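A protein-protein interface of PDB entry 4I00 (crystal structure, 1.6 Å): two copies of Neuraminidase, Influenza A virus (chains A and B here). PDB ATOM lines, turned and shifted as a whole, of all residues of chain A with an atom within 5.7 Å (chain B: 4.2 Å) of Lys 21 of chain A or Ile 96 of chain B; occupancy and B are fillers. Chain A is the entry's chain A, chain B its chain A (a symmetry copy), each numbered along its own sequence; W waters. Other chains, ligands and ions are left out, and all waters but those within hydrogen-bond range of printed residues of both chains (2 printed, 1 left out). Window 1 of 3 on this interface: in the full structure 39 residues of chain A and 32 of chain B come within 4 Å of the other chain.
Of the printed residues of chain B, Pro 18 of chain A touches Ile 96 and Thr 115.
Printed residues of chain B within 4 Å of Lys 21 of chain A: Pro 73, Tyr 74, Ser 76, Glu 93 and Ile 96.
Of the printed residues of chain A, Tyr 74 of chain B touches Lys 21 (3.8 Å), Asn 23 (3.3 Å), Arg 26 (3.5 Å), Pro 378 (3.4 Å) and Gly 380 (3.2 Å).
Of the printed residues of chain A, Ser 76 of chain B touches Lys 21.
Of chain A, only Pro 18 (3.8 Å), Phe 19 (2.9 Å), His 20 (3.7 Å), Lys 21 (3.5 Å) and Trp 377 (3.8 Å) come within 4 Å of Ile 96 of chain B.
Ala 97 of chain B touches none of the printed residues of chain A.
The nearest printed residue of chain B that does not touch Lys 21 of chain A is Cys 95 of chain B (5.5 Å).
No position is printed for both chains.
Of the 20 pairs that touch across the chains among the printed residues, none has its exchanged pair printed and touching as well.
Water W2 lies within hydrogen-bond range of the backbone carbonyl oxygen of Ile 96 of chain B and the backbone carbonyl oxygen of Pro 18 of chain A.
Water W1 lies within hydrogen-bond range of OD1 of Asn 23 of chain A (2.9 Å), OG of Ser 76 of chain B (3.0 Å) and O of Lys 21 of chain A (3.2 Å).
O of Phe 19 of chain A sits at hydrogen-bond distance from N of Ile 96 of chain B (2.9 Å).
The side-chain carboxylate of Glu 93 of chain B lies within hydrogen-bond range of the backbone NH of Lys 21 of chain A.
A ring nitrogen (ND1) of His 20 of chain A lies within hydrogen-bond range of the side-chain carboxylate (OE1) of Glu 93 of chain B (2.6 Å).
The indole nitrogen of Trp 377 of chain A is in hydrogen-bond range of the side-chain hydroxyl of Thr 115 of chain B, 3.0 Å away.
O of Tyr 74 of chain B sits close to OD1 of Asn 23 of chain A, 3.3 Å away.
The side-chain sulfur of Cys 95 of chain B forms a disulfide with the side-chain sulfur of Cys 113 of chain B (2.0 Å).
The backbone carbonyl oxygen (O) of Thr 364 of chain A sits at hydrogen-bond distance from the backbone NH (N) of Phe 19 of chain A (2.9 Å).
NZ of Lys 21 of chain A sits close to ND2 of Asn 23 of chain A, at 2.8 Å.
OG of Ser 76 of chain B is in hydrogen-bond range of OE2 of Glu 93 of chain B.
The side-chain hydroxyl (OG1) of Thr 364 of chain A is in hydrogen-bond range of the backbone carbonyl oxygen (O) of His 20 of chain A (2.8 Å).
NZ of Lys 21 of chain A sits at hydrogen-bond distance from O of Pro 378 of chain A (2.8 Å).
Printed residues of chain B that touch a printed residue of chain A: Pro 73, Tyr 74, Ser 76, Glu 93, Cys 95, Ile 96 and Thr 115.
Printed residues of chain A that touch a printed residue of chain B: Pro 18, Phe 19, His 20, Lys 21, Asn 23, Arg 26, Gly 83, Thr 84, Trp 377, Pro 378 and Gly 380.
Among the printed residues, no Asp or Glu carboxylate lies within 4 Å of a Lys or Arg side-chain nitrogen of the other chain.
Among the printed residues, pairs that only touch across the chains: Pro 18 of chain A with Ile 96 of chain B (3.8 Å), Pro 18 of chain A with Thr 115 of chain B (3.4 Å), Phe 19 of chain A with Cys 95 of chain B (3.2 Å), His 20 of chain A with Ile 96 of chain B (3.7 Å), Lys 21 of chain A with Pro 73 of chain B (3.5 Å), Lys 21 of chain A with Tyr 74 of chain B (3.8 Å), Lys 21 of chain A with Ser 76 of chain B (3.5 Å), Lys 21 of chain A with Ile 96 of chain B (3.5 Å), Arg 26 of chain A with Tyr 74 of chain B (3.5 Å), Gly 83 of chain A with Glu 93 of chain B (3.2 Å), Thr 84 of chain A with Glu 93 of chain B (3.8 Å), Trp 377 of chain A with Pro 73 of chain B (3.7 Å), Trp 377 of chain A with Ile 96 of chain B (3.8 Å), Pro 378 of chain A with Tyr 74 of chain B (3.4 Å) and Gly 380 of chain A with Tyr 74 of chain B (3.2 Å).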
ATOM      1  N   PRO A  18     -23.161 -13.190  22.105  1.00  0.00           N
ATOM      2  CA  PRO A  18     -22.342 -13.784  21.033  1.00  0.00           C
ATOM      3  C   PRO A  18     -22.573 -15.282  20.875  1.00  0.00           C
ATOM      4  O   PRO A  18     -22.547 -16.023  21.852  1.00  0.00           O
ATOM      5  CB  PRO A  18     -20.905 -13.520  21.491  1.00  0.00           C
ATOM      6  CG  PRO A  18     -21.003 -13.328  22.963  1.00  0.00           C
ATOM      7  CD  PRO A  18     -22.345 -12.734  23.247  1.00  0.00           C
ATOM      8  N   PHE A  19     -22.800 -15.706  19.633  1.00  0.00           N
ATOM      9  CA  PHE A  19     -23.211 -17.083  19.338  1.00  0.00           C
ATOM     10  C   PHE A  19     -22.098 -17.827  18.604  1.00  0.00           C
ATOM     11  O   PHE A  19     -21.277 -18.513  19.233  1.00  0.00           O
ATOM     12  CB  PHE A  19     -24.468 -16.982  18.475  1.00  0.00           C
ATOM     13  CG  PHE A  19     -25.255 -18.262  18.314  1.00  0.00           C
ATOM     14  CD1 PHE A  19     -25.177 -19.295  19.225  1.00  0.00           C
ATOM     15  CD2 PHE A  19     -26.132 -18.383  17.239  1.00  0.00           C
ATOM     16  CE1 PHE A  19     -25.935 -20.458  19.046  1.00  0.00           C
ATOM     17  CE2 PHE A  19     -26.894 -19.534  17.062  1.00  0.00           C
ATOM     18  CZ  PHE A  19     -26.796 -20.568  17.958  1.00  0.00           C
ATOM     19  N   HIS A  20     -22.070 -17.669  17.274  1.00  0.00           N
ATOM     20  CA  HIS A  20     -21.068 -18.315  16.421  1.00  0.00           C
ATOM     21  C   HIS A  20     -20.258 -17.252  15.681  1.00  0.00           C
ATOM     22  O   HIS A  20     -20.799 -16.217  15.285  1.00  0.00           O
ATOM     23  CB  HIS A  20     -21.744 -19.198  15.361  1.00  0.00           C
ATOM     24  CG  HIS A  20     -22.397 -20.437  15.893  1.00  0.00           C
ATOM     25  ND1 HIS A  20     -21.725 -21.640  16.026  1.00  0.00           N
ATOM     26  CD2 HIS A  20     -23.681 -20.683  16.258  1.00  0.00           C
ATOM     27  CE1 HIS A  20     -22.564 -22.558  16.478  1.00  0.00           C
ATOM     28  NE2 HIS A  20     -23.753 -22.004  16.628  1.00  0.00           N
ATOM     29  N   LYS A  21     -18.976 -17.520  15.452  1.00  0.00           N
ATOM     30  CA  LYS A  21     -18.142 -16.614  14.660  1.00  0.00           C
ATOM     31  C   LYS A  21     -17.175 -17.438  13.831  1.00  0.00           C
ATOM     32  O   LYS A  21     -16.499 -18.304  14.369  1.00  0.00           O
ATOM     33  CB  LYS A  21     -17.352 -15.679  15.583  1.00  0.00           C
ATOM     34  CG  LYS A  21     -16.538 -14.623  14.842  1.00  0.00           C
ATOM     35  CD  LYS A  21     -15.733 -13.781  15.858  1.00  0.00           C
ATOM     36  CE  LYS A  21     -15.178 -12.511  15.212  1.00  0.00           C
ATOM     37  NZ  LYS A  21     -14.255 -12.812  14.096  1.00  0.00           N
ATOM     38  N   ASP A  22     -17.080 -17.169  12.528  1.00  0.00           N
ATOM     39  CA  ASP A  22     -16.281 -18.061  11.681  1.00  0.00           C
ATOM     40  C   ASP A  22     -14.820 -17.652  11.449  1.00  0.00           C
ATOM     41  O   ASP A  22     -13.998 -18.495  11.148  1.00  0.00           O
ATOM     42  CB  ASP A  22     -16.994 -18.454  10.374  1.00  0.00           C
ATOM     43  CG  ASP A  22     -17.278 -17.276   9.478  1.00  0.00           C
ATOM     44  OD1 ASP A  22     -16.632 -16.222   9.634  1.00  0.00           O
ATOM     45  OD2 ASP A  22     -18.147 -17.417   8.578  1.00  0.00           O
ATOM     46  N   ASN A  23     -14.484 -16.378  11.631  1.00  0.00           N
ATOM     47  CA  ASN A  23     -13.096 -15.980  11.444  1.00  0.00           C
ATOM     48  C   ASN A  23     -12.593 -16.393  10.067  1.00  0.00           C
ATOM     49  O   ASN A  23     -11.432 -16.788   9.906  1.00  0.00           O
ATOM     50  CB  ASN A  23     -12.220 -16.618  12.526  1.00  0.00           C
ATOM     51  CG  ASN A  23     -12.605 -16.174  13.914  1.00  0.00           C
ATOM     52  OD1 ASN A  23     -13.076 -16.967  14.735  1.00  0.00           O
ATOM     53  ND2 ASN A  23     -12.415 -14.896  14.187  1.00  0.00           N
ATOM     54  N   ARG A  26      -9.338 -14.588   8.445  1.00  0.00           N
ATOM     55  CA  ARG A  26      -8.140 -15.036   9.146  1.00  0.00           C
ATOM     56  C   ARG A  26      -7.761 -16.461   8.712  1.00  0.00           C
ATOM     57  O   ARG A  26      -6.611 -16.739   8.366  1.00  0.00           O
ATOM     58  CB  ARG A  26      -8.360 -14.991  10.662  1.00  0.00           C
ATOM     59  CG  ARG A  26      -8.467 -13.584  11.254  1.00  0.00           C
ATOM     60  CD  ARG A  26      -8.973 -13.629  12.687  1.00  0.00           C
ATOM     61  NE  ARG A  26      -8.170 -14.507  13.544  1.00  0.00           N
ATOM     62  CZ  ARG A  26      -7.163 -14.101  14.319  1.00  0.00           C
ATOM     63  NH1 ARG A  26      -6.506 -14.977  15.063  1.00  0.00           N
ATOM     64  NH2 ARG A  26      -6.814 -12.821  14.356  1.00  0.00           N
ATOM     65  N   GLY A  83     -20.669 -21.024  11.631  1.00  0.00           N
ATOM     66  CA  GLY A  83     -19.467 -20.649  12.353  1.00  0.00           C
ATOM     67  C   GLY A  83     -18.196 -21.261  11.786  1.00  0.00           C
ATOM     68  O   GLY A  83     -17.105 -21.033  12.331  1.00  0.00           O
ATOM     69  N   THR A  84     -18.313 -22.052  10.719  1.00  0.00           N
ATOM     70  CA  THR A  84     -17.110 -22.539  10.039  1.00  0.00           C
ATOM     71  C   THR A  84     -16.794 -21.685   8.810  1.00  0.00           C
ATOM     72  O   THR A  84     -17.684 -21.056   8.226  1.00  0.00           O
ATOM     73  CB  THR A  84     -17.196 -24.037   9.600  1.00  0.00           C
ATOM     74  OG1 THR A  84     -18.160 -24.195   8.544  1.00  0.00           O
ATOM     75  CG2 THR A  84     -17.540 -24.940  10.788  1.00  0.00           C
ATOM     76  N   LEU A 344     -19.023  -9.197   7.902  1.00  0.00           N
ATOM     77  CA  LEU A 344     -17.840  -8.384   8.146  1.00  0.00           C
ATOM     78  C   LEU A 344     -17.026  -8.366   6.855  1.00  0.00           C
ATOM     79  O   LEU A 344     -16.237  -9.259   6.584  1.00  0.00           O
ATOM     80  CB  LEU A 344     -17.043  -8.944   9.337  1.00  0.00           C
ATOM     81  CG  LEU A 344     -17.886  -9.210  10.591  1.00  0.00           C
ATOM     82  CD1 LEU A 344     -17.079  -9.934  11.666  1.00  0.00           C
ATOM     83  CD2 LEU A 344     -18.491  -7.932  11.158  1.00  0.00           C
ATOM     84  N   SER A 361     -16.326 -12.248   6.588  1.00  0.00           N
ATOM     85  CA  SER A 361     -16.535 -13.278   7.596  1.00  0.00           C
ATOM     86  C   SER A 361     -17.895 -13.035   8.221  1.00  0.00           C
ATOM     87  O   SER A 361     -18.622 -12.141   7.799  1.00  0.00           O
ATOM     88  CB  SER A 361     -15.421 -13.314   8.655  1.00  0.00           C
ATOM     89  OG  SER A 361     -15.304 -12.092   9.350  1.00  0.00           O
ATOM     90  N   ILE A 362     -18.243 -13.848   9.204  1.00  0.00           N
ATOM     91  CA  ILE A 362     -19.552 -13.786   9.829  1.00  0.00           C
ATOM     92  C   ILE A 362     -19.443 -13.790  11.340  1.00  0.00           C
ATOM     93  O   ILE A 362     -18.604 -14.498  11.919  1.00  0.00           O
ATOM     94  CB  ILE A 362     -20.418 -15.011   9.430  1.00  0.00           C
ATOM     95  CG1 ILE A 362     -20.615 -15.051   7.915  1.00  0.00           C
ATOM     96  CG2 ILE A 362     -21.783 -14.953  10.117  1.00  0.00           C
ATOM     97  CD1 ILE A 362     -21.226 -16.356   7.427  1.00  0.00           C
ATOM     98  N   VAL A 363     -20.300 -13.014  11.988  1.00  0.00           N
ATOM     99  CA  VAL A 363     -20.479 -13.157  13.420  1.00  0.00           C
ATOM    100  C   VAL A 363     -21.978 -13.145  13.705  1.00  0.00           C
ATOM    101  O   VAL A 363     -22.744 -12.555  12.965  1.00  0.00           O
ATOM    102  CB  VAL A 363     -19.743 -12.057  14.198  1.00  0.00           C
ATOM    103  CG1 VAL A 363     -20.352 -10.660  13.888  1.00  0.00           C
ATOM    104  CG2 VAL A 363     -19.741 -12.373  15.698  1.00  0.00           C
ATOM    105  N   THR A 364     -22.393 -13.838  14.752  1.00  0.00           N
ATOM    106  CA  THR A 364     -23.811 -13.957  15.053  1.00  0.00           C
ATOM    107  C   THR A 364     -24.114 -13.722  16.528  1.00  0.00           C
ATOM    108  O   THR A 364     -23.267 -13.949  17.397  1.00  0.00           O
ATOM    109  CB  THR A 364     -24.344 -15.343  14.641  1.00  0.00           C
ATOM    110  OG1 THR A 364     -23.599 -16.358  15.323  1.00  0.00           O
ATOM    111  CG2 THR A 364     -24.179 -15.551  13.139  1.00  0.00           C
ATOM    112  N   TRP A 377     -16.314  -8.144  18.616  1.00  0.00           N
ATOM    113  CA  TRP A 377     -16.093  -9.353  17.826  1.00  0.00           C
ATOM    114  C   TRP A 377     -16.030  -9.017  16.339  1.00  0.00           C
ATOM    115  O   TRP A 377     -16.934  -9.374  15.568  1.00  0.00           O
ATOM    116  CB  TRP A 377     -17.191 -10.385  18.106  1.00  0.00           C
ATOM    117  CG  TRP A 377     -17.230 -10.872  19.530  1.00  0.00           C
ATOM    118  CD1 TRP A 377     -16.535 -11.937  20.067  1.00  0.00           C
ATOM    119  CD2 TRP A 377     -18.013 -10.329  20.597  1.00  0.00           C
ATOM    120  NE1 TRP A 377     -16.842 -12.074  21.403  1.00  0.00           N
ATOM    121  CE2 TRP A 377     -17.742 -11.094  21.753  1.00  0.00           C
ATOM    122  CE3 TRP A 377     -18.910  -9.255  20.690  1.00  0.00           C
ATOM    123  CZ2 TRP A 377     -18.346 -10.828  22.979  1.00  0.00           C
ATOM    124  CZ3 TRP A 377     -19.507  -8.992  21.908  1.00  0.00           C
ATOM    125  CH2 TRP A 377     -19.218  -9.771  23.044  1.00  0.00           C
ATOM    126  N   PRO A 378     -14.950  -8.334  15.924  1.00  0.00           N
ATOM    127  CA  PRO A 378     -14.737  -7.907  14.537  1.00  0.00           C
ATOM    128  C   PRO A 378     -14.115  -9.006  13.690  1.00  0.00           C
ATOM    129  O   PRO A 378     -13.776 -10.071  14.210  1.00  0.00           O
ATOM    130  CB  PRO A 378     -13.724  -6.778  14.687  1.00  0.00           C
ATOM    131  CG  PRO A 378     -12.887  -7.218  15.841  1.00  0.00           C
ATOM    132  CD  PRO A 378     -13.811  -7.967  16.786  1.00  0.00           C
ATOM    133  N   ASP A 379     -13.921  -8.734  12.405  1.00  0.00           N
ATOM    134  CA  ASP A 379     -13.319  -9.718  11.517  1.00  0.00           C
ATOM    135  C   ASP A 379     -11.981 -10.246  12.062  1.00  0.00           C
ATOM    136  O   ASP A 379     -11.725 -11.443  12.070  1.00  0.00           O
ATOM    137  CB  ASP A 379     -13.123  -9.134  10.126  1.00  0.00           C
ATOM    138  CG  ASP A 379     -12.307 -10.040   9.244  1.00  0.00           C
ATOM    139  OD1 ASP A 379     -12.851 -11.058   8.752  1.00  0.00           O
ATOM    140  OD2 ASP A 379     -11.108  -9.759   9.064  1.00  0.00           O
ATOM    141  N   GLY A 380     -11.135  -9.335  12.525  1.00  0.00           N
ATOM    142  CA  GLY A 380      -9.900  -9.708  13.184  1.00  0.00           C
ATOM    143  C   GLY A 380      -8.719  -9.998  12.278  1.00  0.00           C
ATOM    144  O   GLY A 380      -7.633 -10.306  12.770  1.00  0.00           O
ATOM    145  N   PRO B  73     -11.277 -12.305  20.779  1.00  0.00           N
ATOM    146  CA  PRO B  73     -12.622 -12.500  20.221  1.00  0.00           C
ATOM    147  C   PRO B  73     -12.645 -13.572  19.124  1.00  0.00           C
ATOM    148  O   PRO B  73     -13.729 -13.962  18.678  1.00  0.00           O
ATOM    149  CB  PRO B  73     -12.957 -11.124  19.614  1.00  0.00           C
ATOM    150  CG  PRO B  73     -11.981 -10.154  20.257  1.00  0.00           C
ATOM    151  CD  PRO B  73     -10.736 -10.964  20.494  1.00  0.00           C
ATOM    152  N   TYR B  74     -11.465 -14.030  18.703  1.00  0.00           N
ATOM    153  CA  TYR B  74     -11.315 -14.917  17.549  1.00  0.00           C
ATOM    154  C   TYR B  74     -11.164 -16.355  17.996  1.00  0.00           C
ATOM    155  O   TYR B  74     -10.863 -17.222  17.182  1.00  0.00           O
ATOM    156  CB  TYR B  74     -10.101 -14.490  16.716  1.00  0.00           C
ATOM    157  CG  TYR B  74     -10.015 -12.978  16.618  1.00  0.00           C
ATOM    158  CD1 TYR B  74     -11.044 -12.243  16.049  1.00  0.00           C
ATOM    159  CD2 TYR B  74      -8.929 -12.286  17.148  1.00  0.00           C
ATOM    160  CE1 TYR B  74     -10.989 -10.861  15.992  1.00  0.00           C
ATOM    161  CE2 TYR B  74      -8.864 -10.906  17.086  1.00  0.00           C
ATOM    162  CZ  TYR B  74      -9.893 -10.204  16.511  1.00  0.00           C
ATOM    163  OH  TYR B  74      -9.836  -8.830  16.445  1.00  0.00           O
ATOM    164  N   ARG B  75     -11.361 -16.596  19.289  1.00  0.00           N
ATOM    165  CA  ARG B  75     -11.343 -17.955  19.809  1.00  0.00           C
ATOM    166  C   ARG B  75     -12.756 -18.522  19.842  1.00  0.00           C
ATOM    167  O   ARG B  75     -13.691 -17.860  20.291  1.00  0.00           O
ATOM    168  CB  ARG B  75     -10.704 -18.014  21.202  1.00  0.00           C
ATOM    169  CG  ARG B  75      -9.266 -17.530  21.207  1.00  0.00           C
ATOM    170  CD  ARG B  75      -8.505 -18.081  22.401  1.00  0.00           C
ATOM    171  NE  ARG B  75      -8.132 -19.482  22.192  1.00  0.00           N
ATOM    172  CZ  ARG B  75      -7.386 -20.186  23.036  1.00  0.00           C
ATOM    173  NH1 ARG B  75      -6.943 -19.614  24.150  1.00  0.00           N
ATOM    174  NH2 ARG B  75      -7.080 -21.458  22.771  1.00  0.00           N
ATOM    175  N   SER B  76     -12.892 -19.748  19.329  1.00  0.00           N
ATOM    176  CA  SER B  76     -14.145 -20.491  19.343  1.00  0.00           C
ATOM    177  C   SER B  76     -13.924 -21.881  19.904  1.00  0.00           C
ATOM    178  O   SER B  76     -12.886 -22.498  19.669  1.00  0.00           O
ATOM    179  CB  SER B  76     -14.695 -20.676  17.925  1.00  0.00           C
ATOM    180  OG  SER B  76     -15.169 -19.462  17.399  1.00  0.00           O
ATOM    181  N   GLU B  93     -17.827 -25.529  14.506  1.00  0.00           N
ATOM    182  CA  GLU B  93     -17.681 -24.440  15.470  1.00  0.00           C
ATOM    183  C   GLU B  93     -18.896 -24.451  16.396  1.00  0.00           C
ATOM    184  O   GLU B  93     -20.040 -24.351  15.939  1.00  0.00           O
ATOM    185  CB  GLU B  93     -17.523 -23.095  14.760  1.00  0.00           C
ATOM    186  CG  GLU B  93     -17.023 -21.947  15.701  1.00  0.00           C
ATOM    187  CD  GLU B  93     -18.084 -20.907  16.037  1.00  0.00           C
ATOM    188  OE1 GLU B  93     -19.267 -21.061  15.663  1.00  0.00           O
ATOM    189  OE2 GLU B  93     -17.722 -19.904  16.679  1.00  0.00           O
ATOM    190  N   CYS B  95     -19.319 -22.553  19.499  1.00  0.00           N
ATOM    191  CA  CYS B  95     -19.680 -21.225  19.977  1.00  0.00           C
ATOM    192  C   CYS B  95     -18.419 -20.372  20.104  1.00  0.00           C
ATOM    193  O   CYS B  95     -17.303 -20.897  20.104  1.00  0.00           O
ATOM    194  CB  CYS B  95     -20.332 -21.342  21.342  1.00  0.00           C
ATOM    195  SG  CYS B  95     -19.201 -22.221  22.487  1.00  0.00           S
ATOM    196  N   ILE B  96     -18.602 -19.057  20.205  1.00  0.00           N
ATOM    197  CA  ILE B  96     -17.487 -18.159  20.474  1.00  0.00           C
ATOM    198  C   ILE B  96     -17.101 -18.369  21.921  1.00  0.00           C
ATOM    199  O   ILE B  96     -17.956 -18.320  22.803  1.00  0.00           O
ATOM    200  CB  ILE B  96     -17.898 -16.696  20.231  1.00  0.00           C
ATOM    201  CG1 ILE B  96     -18.429 -16.537  18.799  1.00  0.00           C
ATOM    202  CG2 ILE B  96     -16.717 -15.767  20.453  1.00  0.00           C
ATOM    203  CD1 ILE B  96     -19.193 -15.261  18.588  1.00  0.00           C
ATOM    204  N   ALA B  97     -15.826 -18.670  22.170  1.00  0.00           N
ATOM    205  CA  ALA B  97     -15.380 -18.961  23.538  1.00  0.00           C
ATOM    206  C   ALA B  97     -13.883 -18.854  23.719  1.00  0.00           C
ATOM    207  O   ALA B  97     -13.112 -19.323  22.876  1.00  0.00           O
ATOM    208  CB  ALA B  97     -15.846 -20.357  23.973  1.00  0.00           C
ATOM    209  N   CYS B 113     -19.968 -21.365  27.203  1.00  0.00           N
ATOM    210  CA  CYS B 113     -19.013 -20.627  26.368  1.00  0.00           C
ATOM    211  C   CYS B 113     -18.766 -19.209  26.890  1.00  0.00           C
ATOM    212  O   CYS B 113     -19.659 -18.362  26.819  1.00  0.00           O
ATOM    213  CB  CYS B 113     -19.563 -20.532  24.950  1.00  0.00           C
ATOM    214  SG  CYS B 113     -20.079 -22.155  24.315  1.00  0.00           S
ATOM    215  N   THR B 115     -17.031 -15.504  26.601  1.00  0.00           N
ATOM    216  CA  THR B 115     -16.306 -14.602  25.719  1.00  0.00           C
ATOM    217  C   THR B 115     -16.613 -13.143  26.089  1.00  0.00           C
ATOM    218  O   THR B 115     -17.457 -12.874  26.949  1.00  0.00           O
ATOM    219  CB  THR B 115     -16.604 -14.901  24.216  1.00  0.00           C
ATOM    220  OG1 THR B 115     -15.793 -14.078  23.356  1.00  0.00           O
ATOM    221  CG2 THR B 115     -18.075 -14.661  23.913  1.00  0.00           C
HETATM  222  O   HOH W   1     -13.710 -19.819  14.837  1.00  0.00           O
HETATM  223  O   HOH W   2     -20.666 -17.837  23.197  1.00  0.00           O
